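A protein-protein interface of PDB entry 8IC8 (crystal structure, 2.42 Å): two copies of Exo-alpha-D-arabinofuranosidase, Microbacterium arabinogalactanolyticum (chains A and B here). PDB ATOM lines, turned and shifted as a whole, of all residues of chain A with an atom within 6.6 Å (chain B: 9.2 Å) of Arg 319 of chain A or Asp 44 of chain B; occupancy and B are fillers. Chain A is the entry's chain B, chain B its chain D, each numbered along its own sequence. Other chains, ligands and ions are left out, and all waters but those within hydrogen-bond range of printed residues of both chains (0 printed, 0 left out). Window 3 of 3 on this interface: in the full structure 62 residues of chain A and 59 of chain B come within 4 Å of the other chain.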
ATOM      1  N   LEU A 191      32.831 -15.307  21.278  1.00  0.00           N
ATOM      2  CA  LEU A 191      31.587 -15.785  21.882  1.00  0.00           C
ATOM      3  C   LEU A 191      30.776 -14.654  22.508  1.00  0.00           C
ATOM      4  O   LEU A 191      30.305 -14.752  23.645  1.00  0.00           O
ATOM      5  CB  LEU A 191      31.862 -16.881  22.916  1.00  0.00           C
ATOM      6  CG  LEU A 191      31.979 -18.299  22.367  1.00  0.00           C
ATOM      7  CD1 LEU A 191      32.272 -19.280  23.477  1.00  0.00           C
ATOM      8  CD2 LEU A 191      30.721 -18.701  21.613  1.00  0.00           C
ATOM      9  N   GLY A 313      30.375 -19.353  12.428  1.00  0.00           N
ATOM     10  CA  GLY A 313      30.689 -20.063  11.207  1.00  0.00           C
ATOM     11  C   GLY A 313      30.910 -21.535  11.510  1.00  0.00           C
ATOM     12  O   GLY A 313      30.235 -22.082  12.389  1.00  0.00           O
ATOM     13  N   TRP A 314      31.855 -22.187  10.823  1.00  0.00           N
ATOM     14  CA  TRP A 314      32.121 -23.607  11.018  1.00  0.00           C
ATOM     15  C   TRP A 314      33.602 -23.866  11.281  1.00  0.00           C
ATOM     16  O   TRP A 314      34.477 -23.165  10.771  1.00  0.00           O
ATOM     17  CB  TRP A 314      31.669 -24.427   9.807  1.00  0.00           C
ATOM     18  CG  TRP A 314      30.178 -24.425   9.638  1.00  0.00           C
ATOM     19  CD1 TRP A 314      29.447 -23.670   8.765  1.00  0.00           C
ATOM     20  CD2 TRP A 314      29.228 -25.212  10.379  1.00  0.00           C
ATOM     21  NE1 TRP A 314      28.113 -23.944   8.910  1.00  0.00           N
ATOM     22  CE2 TRP A 314      27.949 -24.884   9.894  1.00  0.00           C
ATOM     23  CE3 TRP A 314      29.343 -26.157  11.401  1.00  0.00           C
ATOM     24  CZ2 TRP A 314      26.795 -25.471  10.386  1.00  0.00           C
ATOM     25  CZ3 TRP A 314      28.202 -26.741  11.891  1.00  0.00           C
ATOM     26  CH2 TRP A 314      26.938 -26.399  11.385  1.00  0.00           C
ATOM     27  N   ARG A 315      33.868 -24.875  12.103  1.00  0.00           N
ATOM     28  CA  ARG A 315      35.201 -25.426  12.293  1.00  0.00           C
ATOM     29  C   ARG A 315      35.082 -26.946  12.238  1.00  0.00           C
ATOM     30  O   ARG A 315      33.982 -27.503  12.170  1.00  0.00           O
ATOM     31  CB  ARG A 315      35.842 -24.932  13.608  1.00  0.00           C
ATOM     32  CG  ARG A 315      35.434 -25.658  14.873  1.00  0.00           C
ATOM     33  CD  ARG A 315      36.058 -25.025  16.125  1.00  0.00           C
ATOM     34  NE  ARG A 315      37.480 -24.779  15.942  1.00  0.00           N
ATOM     35  CZ  ARG A 315      38.207 -23.891  16.619  1.00  0.00           C
ATOM     36  NH1 ARG A 315      37.667 -23.148  17.569  1.00  0.00           N
ATOM     37  NH2 ARG A 315      39.492 -23.745  16.335  1.00  0.00           N
ATOM     38  N   SER A 316      36.222 -27.623  12.243  1.00  0.00           N
ATOM     39  CA  SER A 316      36.246 -29.055  11.989  1.00  0.00           C
ATOM     40  C   SER A 316      35.405 -29.832  13.007  1.00  0.00           C
ATOM     41  O   SER A 316      35.259 -29.441  14.170  1.00  0.00           O
ATOM     42  CB  SER A 316      37.686 -29.550  12.014  1.00  0.00           C
ATOM     43  OG  SER A 316      38.224 -29.414  13.312  1.00  0.00           O
ATOM     44  N   GLY A 317      34.872 -30.965  12.558  1.00  0.00           N
ATOM     45  CA  GLY A 317      34.025 -31.780  13.401  1.00  0.00           C
ATOM     46  C   GLY A 317      32.604 -31.278  13.502  1.00  0.00           C
ATOM     47  O   GLY A 317      31.928 -31.560  14.497  1.00  0.00           O
ATOM     48  N   TRP A 318      32.136 -30.524  12.504  1.00  0.00           N
ATOM     49  CA  TRP A 318      30.792 -29.948  12.510  1.00  0.00           C
ATOM     50  C   TRP A 318      30.524 -29.163  13.800  1.00  0.00           C
ATOM     51  O   TRP A 318      29.484 -29.311  14.451  1.00  0.00           O
ATOM     52  CB  TRP A 318      29.742 -31.037  12.286  1.00  0.00           C
ATOM     53  CG  TRP A 318      29.751 -31.565  10.879  1.00  0.00           C
ATOM     54  CD1 TRP A 318      30.402 -32.677  10.423  1.00  0.00           C
ATOM     55  CD2 TRP A 318      29.095 -30.986   9.736  1.00  0.00           C
ATOM     56  NE1 TRP A 318      30.188 -32.830   9.075  1.00  0.00           N
ATOM     57  CE2 TRP A 318      29.386 -31.809   8.627  1.00  0.00           C
ATOM     58  CE3 TRP A 318      28.284 -29.855   9.546  1.00  0.00           C
ATOM     59  CZ2 TRP A 318      28.897 -31.541   7.348  1.00  0.00           C
ATOM     60  CZ3 TRP A 318      27.801 -29.590   8.265  1.00  0.00           C
ATOM     61  CH2 TRP A 318      28.117 -30.426   7.188  1.00  0.00           C
ATOM     62  N   ARG A 319      31.478 -28.314  14.173  1.00  0.00           N
ATOM     63  CA  ARG A 319      31.352 -27.456  15.345  1.00  0.00           C
ATOM     64  C   ARG A 319      31.105 -26.028  14.883  1.00  0.00           C
ATOM     65  O   ARG A 319      31.677 -25.590  13.881  1.00  0.00           O
ATOM     66  CB  ARG A 319      32.618 -27.511  16.221  1.00  0.00           C
ATOM     67  CG  ARG A 319      32.721 -28.735  17.139  1.00  0.00           C
ATOM     68  CD  ARG A 319      34.072 -28.788  17.873  1.00  0.00           C
ATOM     69  NE  ARG A 319      35.191 -28.855  16.935  1.00  0.00           N
ATOM     70  CZ  ARG A 319      36.420 -28.400  17.175  1.00  0.00           C
ATOM     71  NH1 ARG A 319      36.722 -27.844  18.345  1.00  0.00           N
ATOM     72  NH2 ARG A 319      37.356 -28.500  16.235  1.00  0.00           N
ATOM     73  N   TYR A 320      30.246 -25.300  15.592  1.00  0.00           N
ATOM     74  CA  TYR A 320      30.141 -23.872  15.313  1.00  0.00           C
ATOM     75  C   TYR A 320      31.485 -23.211  15.595  1.00  0.00           C
ATOM     76  O   TYR A 320      32.192 -23.594  16.524  1.00  0.00           O
ATOM     77  CB  TYR A 320      29.038 -23.208  16.153  1.00  0.00           C
ATOM     78  CG  TYR A 320      27.633 -23.674  15.843  1.00  0.00           C
ATOM     79  CD1 TYR A 320      27.200 -23.838  14.529  1.00  0.00           C
ATOM     80  CD2 TYR A 320      26.730 -23.949  16.874  1.00  0.00           C
ATOM     81  CE1 TYR A 320      25.916 -24.262  14.245  1.00  0.00           C
ATOM     82  CE2 TYR A 320      25.439 -24.378  16.604  1.00  0.00           C
ATOM     83  CZ  TYR A 320      25.034 -24.529  15.287  1.00  0.00           C
ATOM     84  OH  TYR A 320      23.751 -24.967  15.026  1.00  0.00           O
ATOM     85  N   LEU A 321      31.846 -22.225  14.778  1.00  0.00           N
ATOM     86  CA  LEU A 321      33.085 -21.485  14.987  1.00  0.00           C
ATOM     87  C   LEU A 321      32.751 -20.055  15.377  1.00  0.00           C
ATOM     88  O   LEU A 321      32.184 -19.319  14.552  1.00  0.00           O
ATOM     89  CB  LEU A 321      33.955 -21.503  13.724  1.00  0.00           C
ATOM     90  CG  LEU A 321      35.193 -20.585  13.735  1.00  0.00           C
ATOM     91  CD1 LEU A 321      36.221 -21.042  14.753  1.00  0.00           C
ATOM     92  CD2 LEU A 321      35.816 -20.467  12.348  1.00  0.00           C
ATOM     93  N   GLY B  38      20.969 -28.490  16.544  1.00  0.00           N
ATOM     94  CA  GLY B  38      22.241 -27.818  16.715  1.00  0.00           C
ATOM     95  C   GLY B  38      23.023 -28.187  17.963  1.00  0.00           C
ATOM     96  O   GLY B  38      24.084 -27.593  18.202  1.00  0.00           O
ATOM     97  N   ALA B  39      22.546 -29.161  18.759  1.00  0.00           N
ATOM     98  CA  ALA B  39      23.143 -29.438  20.066  1.00  0.00           C
ATOM     99  C   ALA B  39      24.598 -29.873  19.943  1.00  0.00           C
ATOM    100  O   ALA B  39      25.473 -29.305  20.600  1.00  0.00           O
ATOM    101  CB  ALA B  39      22.333 -30.501  20.809  1.00  0.00           C
ATOM    102  N   ASP B  40      24.876 -30.884  19.106  1.00  0.00           N
ATOM    103  CA  ASP B  40      26.250 -31.357  18.944  1.00  0.00           C
ATOM    104  C   ASP B  40      27.144 -30.286  18.338  1.00  0.00           C
ATOM    105  O   ASP B  40      28.319 -30.174  18.706  1.00  0.00           O
ATOM    106  CB  ASP B  40      26.298 -32.606  18.067  1.00  0.00           C
ATOM    107  CG  ASP B  40      25.545 -33.761  18.656  1.00  0.00           C
ATOM    108  OD1 ASP B  40      25.567 -33.913  19.902  1.00  0.00           O
ATOM    109  OD2 ASP B  40      24.932 -34.518  17.866  1.00  0.00           O
ATOM    110  N   CYS B  41      26.611 -29.506  17.393  1.00  0.00           N
ATOM    111  CA  CYS B  41      27.381 -28.421  16.801  1.00  0.00           C
ATOM    112  C   CYS B  41      27.823 -27.416  17.847  1.00  0.00           C
ATOM    113  O   CYS B  41      28.828 -26.716  17.653  1.00  0.00           O
ATOM    114  CB  CYS B  41      26.563 -27.705  15.718  1.00  0.00           C
ATOM    115  SG  CYS B  41      25.970 -28.777  14.402  1.00  0.00           S
ATOM    116  N   ALA B  42      27.108 -27.330  18.957  1.00  0.00           N
ATOM    117  CA  ALA B  42      27.480 -26.391  19.994  1.00  0.00           C
ATOM    118  C   ALA B  42      28.173 -27.060  21.178  1.00  0.00           C
ATOM    119  O   ALA B  42      28.317 -26.425  22.222  1.00  0.00           O
ATOM    120  CB  ALA B  42      26.236 -25.625  20.456  1.00  0.00           C
ATOM    121  N   ARG B  43      28.616 -28.315  21.037  1.00  0.00           N
ATOM    122  CA  ARG B  43      29.148 -29.039  22.194  1.00  0.00           C
ATOM    123  C   ARG B  43      30.296 -28.295  22.870  1.00  0.00           C
ATOM    124  O   ARG B  43      30.436 -28.366  24.093  1.00  0.00           O
ATOM    125  CB  ARG B  43      29.593 -30.451  21.799  1.00  0.00           C
ATOM    126  CG  ARG B  43      30.701 -30.569  20.743  1.00  0.00           C
ATOM    127  CD  ARG B  43      30.726 -32.017  20.236  1.00  0.00           C
ATOM    128  NE  ARG B  43      31.739 -32.261  19.226  1.00  0.00           N
ATOM    129  CZ  ARG B  43      31.576 -32.048  17.924  1.00  0.00           C
ATOM    130  NH1 ARG B  43      30.407 -31.622  17.465  1.00  0.00           N
ATOM    131  NH2 ARG B  43      32.579 -32.273  17.075  1.00  0.00           N
ATOM    132  N   ASP B  44      31.119 -27.565  22.113  1.00  0.00           N
ATOM    133  CA  ASP B  44      32.176 -26.803  22.761  1.00  0.00           C
ATOM    134  C   ASP B  44      31.679 -25.496  23.368  1.00  0.00           C
ATOM    135  O   ASP B  44      32.387 -24.908  24.192  1.00  0.00           O
ATOM    136  CB  ASP B  44      33.300 -26.512  21.770  1.00  0.00           C
ATOM    137  CG  ASP B  44      34.145 -27.736  21.472  1.00  0.00           C
ATOM    138  OD1 ASP B  44      33.907 -28.815  22.068  1.00  0.00           O
ATOM    139  OD2 ASP B  44      35.061 -27.610  20.636  1.00  0.00           O
ATOM    140  N   LEU B  45      30.501 -25.017  22.978  1.00  0.00           N
ATOM    141  CA  LEU B  45      29.943 -23.772  23.497  1.00  0.00           C
ATOM    142  C   LEU B  45      28.769 -24.091  24.427  1.00  0.00           C
ATOM    143  O   LEU B  45      28.309 -25.228  24.524  1.00  0.00           O
ATOM    144  CB  LEU B  45      29.525 -22.867  22.332  1.00  0.00           C
ATOM    145  CG  LEU B  45      30.359 -23.046  21.042  1.00  0.00           C
ATOM    146  CD1 LEU B  45      29.766 -22.300  19.854  1.00  0.00           C
ATOM    147  CD2 LEU B  45      31.788 -22.583  21.236  1.00  0.00           C
ATOM    148  N   GLY B  46      28.273 -23.098  25.145  1.00  0.00           N
ATOM    149  CA  GLY B  46      27.173 -23.360  26.057  1.00  0.00           C
ATOM    150  C   GLY B  46      25.886 -23.752  25.345  1.00  0.00           C
ATOM    151  O   GLY B  46      25.884 -24.065  24.149  1.00  0.00           O
ATOM    152  N   PRO B  47      24.771 -23.791  26.073  1.00  0.00           N
ATOM    153  CA  PRO B  47      23.474 -23.572  25.422  1.00  0.00           C
ATOM    154  C   PRO B  47      23.308 -22.093  25.097  1.00  0.00           C
ATOM    155  O   PRO B  47      24.106 -21.244  25.494  1.00  0.00           O
ATOM    156  CB  PRO B  47      22.453 -24.066  26.456  1.00  0.00           C
ATOM    157  CG  PRO B  47      23.227 -25.086  27.262  1.00  0.00           C
ATOM    158  CD  PRO B  47      24.611 -24.469  27.373  1.00  0.00           C
ATOM    159  N   TRP B  49      23.609 -21.231  21.975  1.00  0.00           N
ATOM    160  CA  TRP B  49      24.389 -21.059  20.745  1.00  0.00           C
ATOM    161  C   TRP B  49      23.836 -21.972  19.654  1.00  0.00           C
ATOM    162  O   TRP B  49      24.427 -22.994  19.305  1.00  0.00           O
ATOM    163  CB  TRP B  49      25.888 -21.308  21.005  1.00  0.00           C
ATOM    164  CG  TRP B  49      26.500 -20.224  21.854  1.00  0.00           C
ATOM    165  CD1 TRP B  49      26.775 -20.286  23.196  1.00  0.00           C
ATOM    166  CD2 TRP B  49      26.893 -18.911  21.425  1.00  0.00           C
ATOM    167  NE1 TRP B  49      27.322 -19.095  23.620  1.00  0.00           N
ATOM    168  CE2 TRP B  49      27.400 -18.233  22.557  1.00  0.00           C
ATOM    169  CE3 TRP B  49      26.858 -18.241  20.199  1.00  0.00           C
ATOM    170  CZ2 TRP B  49      27.871 -16.916  22.497  1.00  0.00           C
ATOM    171  CZ3 TRP B  49      27.326 -16.934  20.134  1.00  0.00           C
ATOM    172  CH2 TRP B  49      27.826 -16.283  21.277  1.00  0.00           C
ATOM    173  N   ILE B  51      21.039 -23.993  19.270  1.00  0.00           N
ATOM    174  CA  ILE B  51      20.823 -25.373  19.694  1.00  0.00           C
ATOM    175  C   ILE B  51      19.719 -26.028  18.875  1.00  0.00           C
ATOM    176  O   ILE B  51      19.699 -27.259  18.716  1.00  0.00           O
ATOM    177  CB  ILE B  51      20.501 -25.424  21.205  1.00  0.00           C
ATOM    178  CG1 ILE B  51      21.590 -24.734  22.036  1.00  0.00           C
ATOM    179  CG2 ILE B  51      20.302 -26.856  21.683  1.00  0.00           C
ATOM    180  CD1 ILE B  51      22.955 -25.287  21.812  1.00  0.00           C
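NH1 of Arg 319 of chain A lies within salt-bridge range of OD2 of Asp 44 of chain B (2.8 Å). The backbone carbonyl oxygen of Gly 317 of chain A lies within hydrogen-bond range of the guanidinium group of Arg 43 of chain B (2.8 Å). SG of Cys 41 of chain B lies close to O of Trp 318 of chain A (3.6 Å). The backbone carbonyl oxygen (O) of Cys 41 of chain B is in hydrogen-bond range of the backbone NH (N) of Tyr 320 of chain A, at 2.9 Å.
The backbone NH of Gly 38 of chain B sits at hydrogen-bond distance from the backbone carbonyl oxygen of Ile 51 of chain B (2.8 Å). O of Ser 316 of chain A lies within hydrogen-bond range of NE of Arg 319 of chain A, at 2.8 Å. The guanidinium group (NH1) of Arg 43 of chain B lies within hydrogen-bond range of the backbone carbonyl oxygen (O) of Asp 40 of chain B (2.8 Å).
Leu 191 of chain A touches Trp 49 of chain B (O to CZ2, 3.5 Å). SG of Cys 41 of chain B touches CZ3 of Trp 314 of chain A (3.9 Å). O of Trp 318 of chain A touches NH1 of Arg 43 of chain B, 3.9 Å away. Cys 41 of chain B touches Arg 319 of chain A (O to CA, 3.5 Å). CG of Arg 319 of chain A touches NH2 of Arg 43 of chain B, at 3.5 Å. Gly 38 of chain B touches Tyr 320 of chain A (CA to OH, 3.6 Å). Tyr 320 of chain A touches Ala 42 of chain B. CB of Tyr 320 of chain A touches CD1 of Leu 45 of chain B, at 3.9 Å. Trp 49 of chain B touches Tyr 320 of chain A (O to CE2, 3.2 Å).
Of chain B, only Cys 41, Arg 43 and Asp 44 come within 4 Å of Arg 319 of chain A. Of the printed residues of chain A, Asp 44 of chain B touches Arg 319 (2.8 Å). No residue of chain B comes within 4 Å of Ser 316 of chain A. Of the printed residues of chain B, Leu 191 of chain A touches Trp 49. Of the printed residues of chain B, Tyr 320 of chain A touches Gly 38 (3.6 Å), Cys 41 (2.9 Å), Ala 42 (3.99 Å), Leu 45 (3.9 Å) and Trp 49 (3.2 Å). The nearest printed residue of chain B that does not touch Leu 191 of chain A is Leu 45 of chain B (4.02 Å).
Printed residues of chain B that touch a printed residue of chain A: Gly 38, Cys 41, Ala 42, Arg 43, Asp 44, Leu 45 and Trp 49. Hydrophobic or aromatic side chains of chain B that line the printed part of chain A: Ala 42, Leu 45 and Trp 49. Of the 10 printed residues of chain A, 6 touch a printed residue of chain B. Printed residues of chain A that touch a printed residue of chain B: Leu 191, Trp 314, Gly 317, Trp 318, Arg 319 and Tyr 320. Hydrophobic or aromatic side chains of chain A that line the printed part of chain B: Leu 191, Trp 314 and Tyr 320. Among the printed residues, 13 pairs touch across the chains. Among the printed residues, Asp or Glu carboxylates within 4 Å of a Lys or Arg side-chain nitrogen of the other chain: Arg 319 of chain A with Asp 44 of chain B (2.8 Å).
No position is printed for both chains. Of the 13 pairs that touch across the chains among the printed residues, none has its exchanged pair printed and touching as well.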
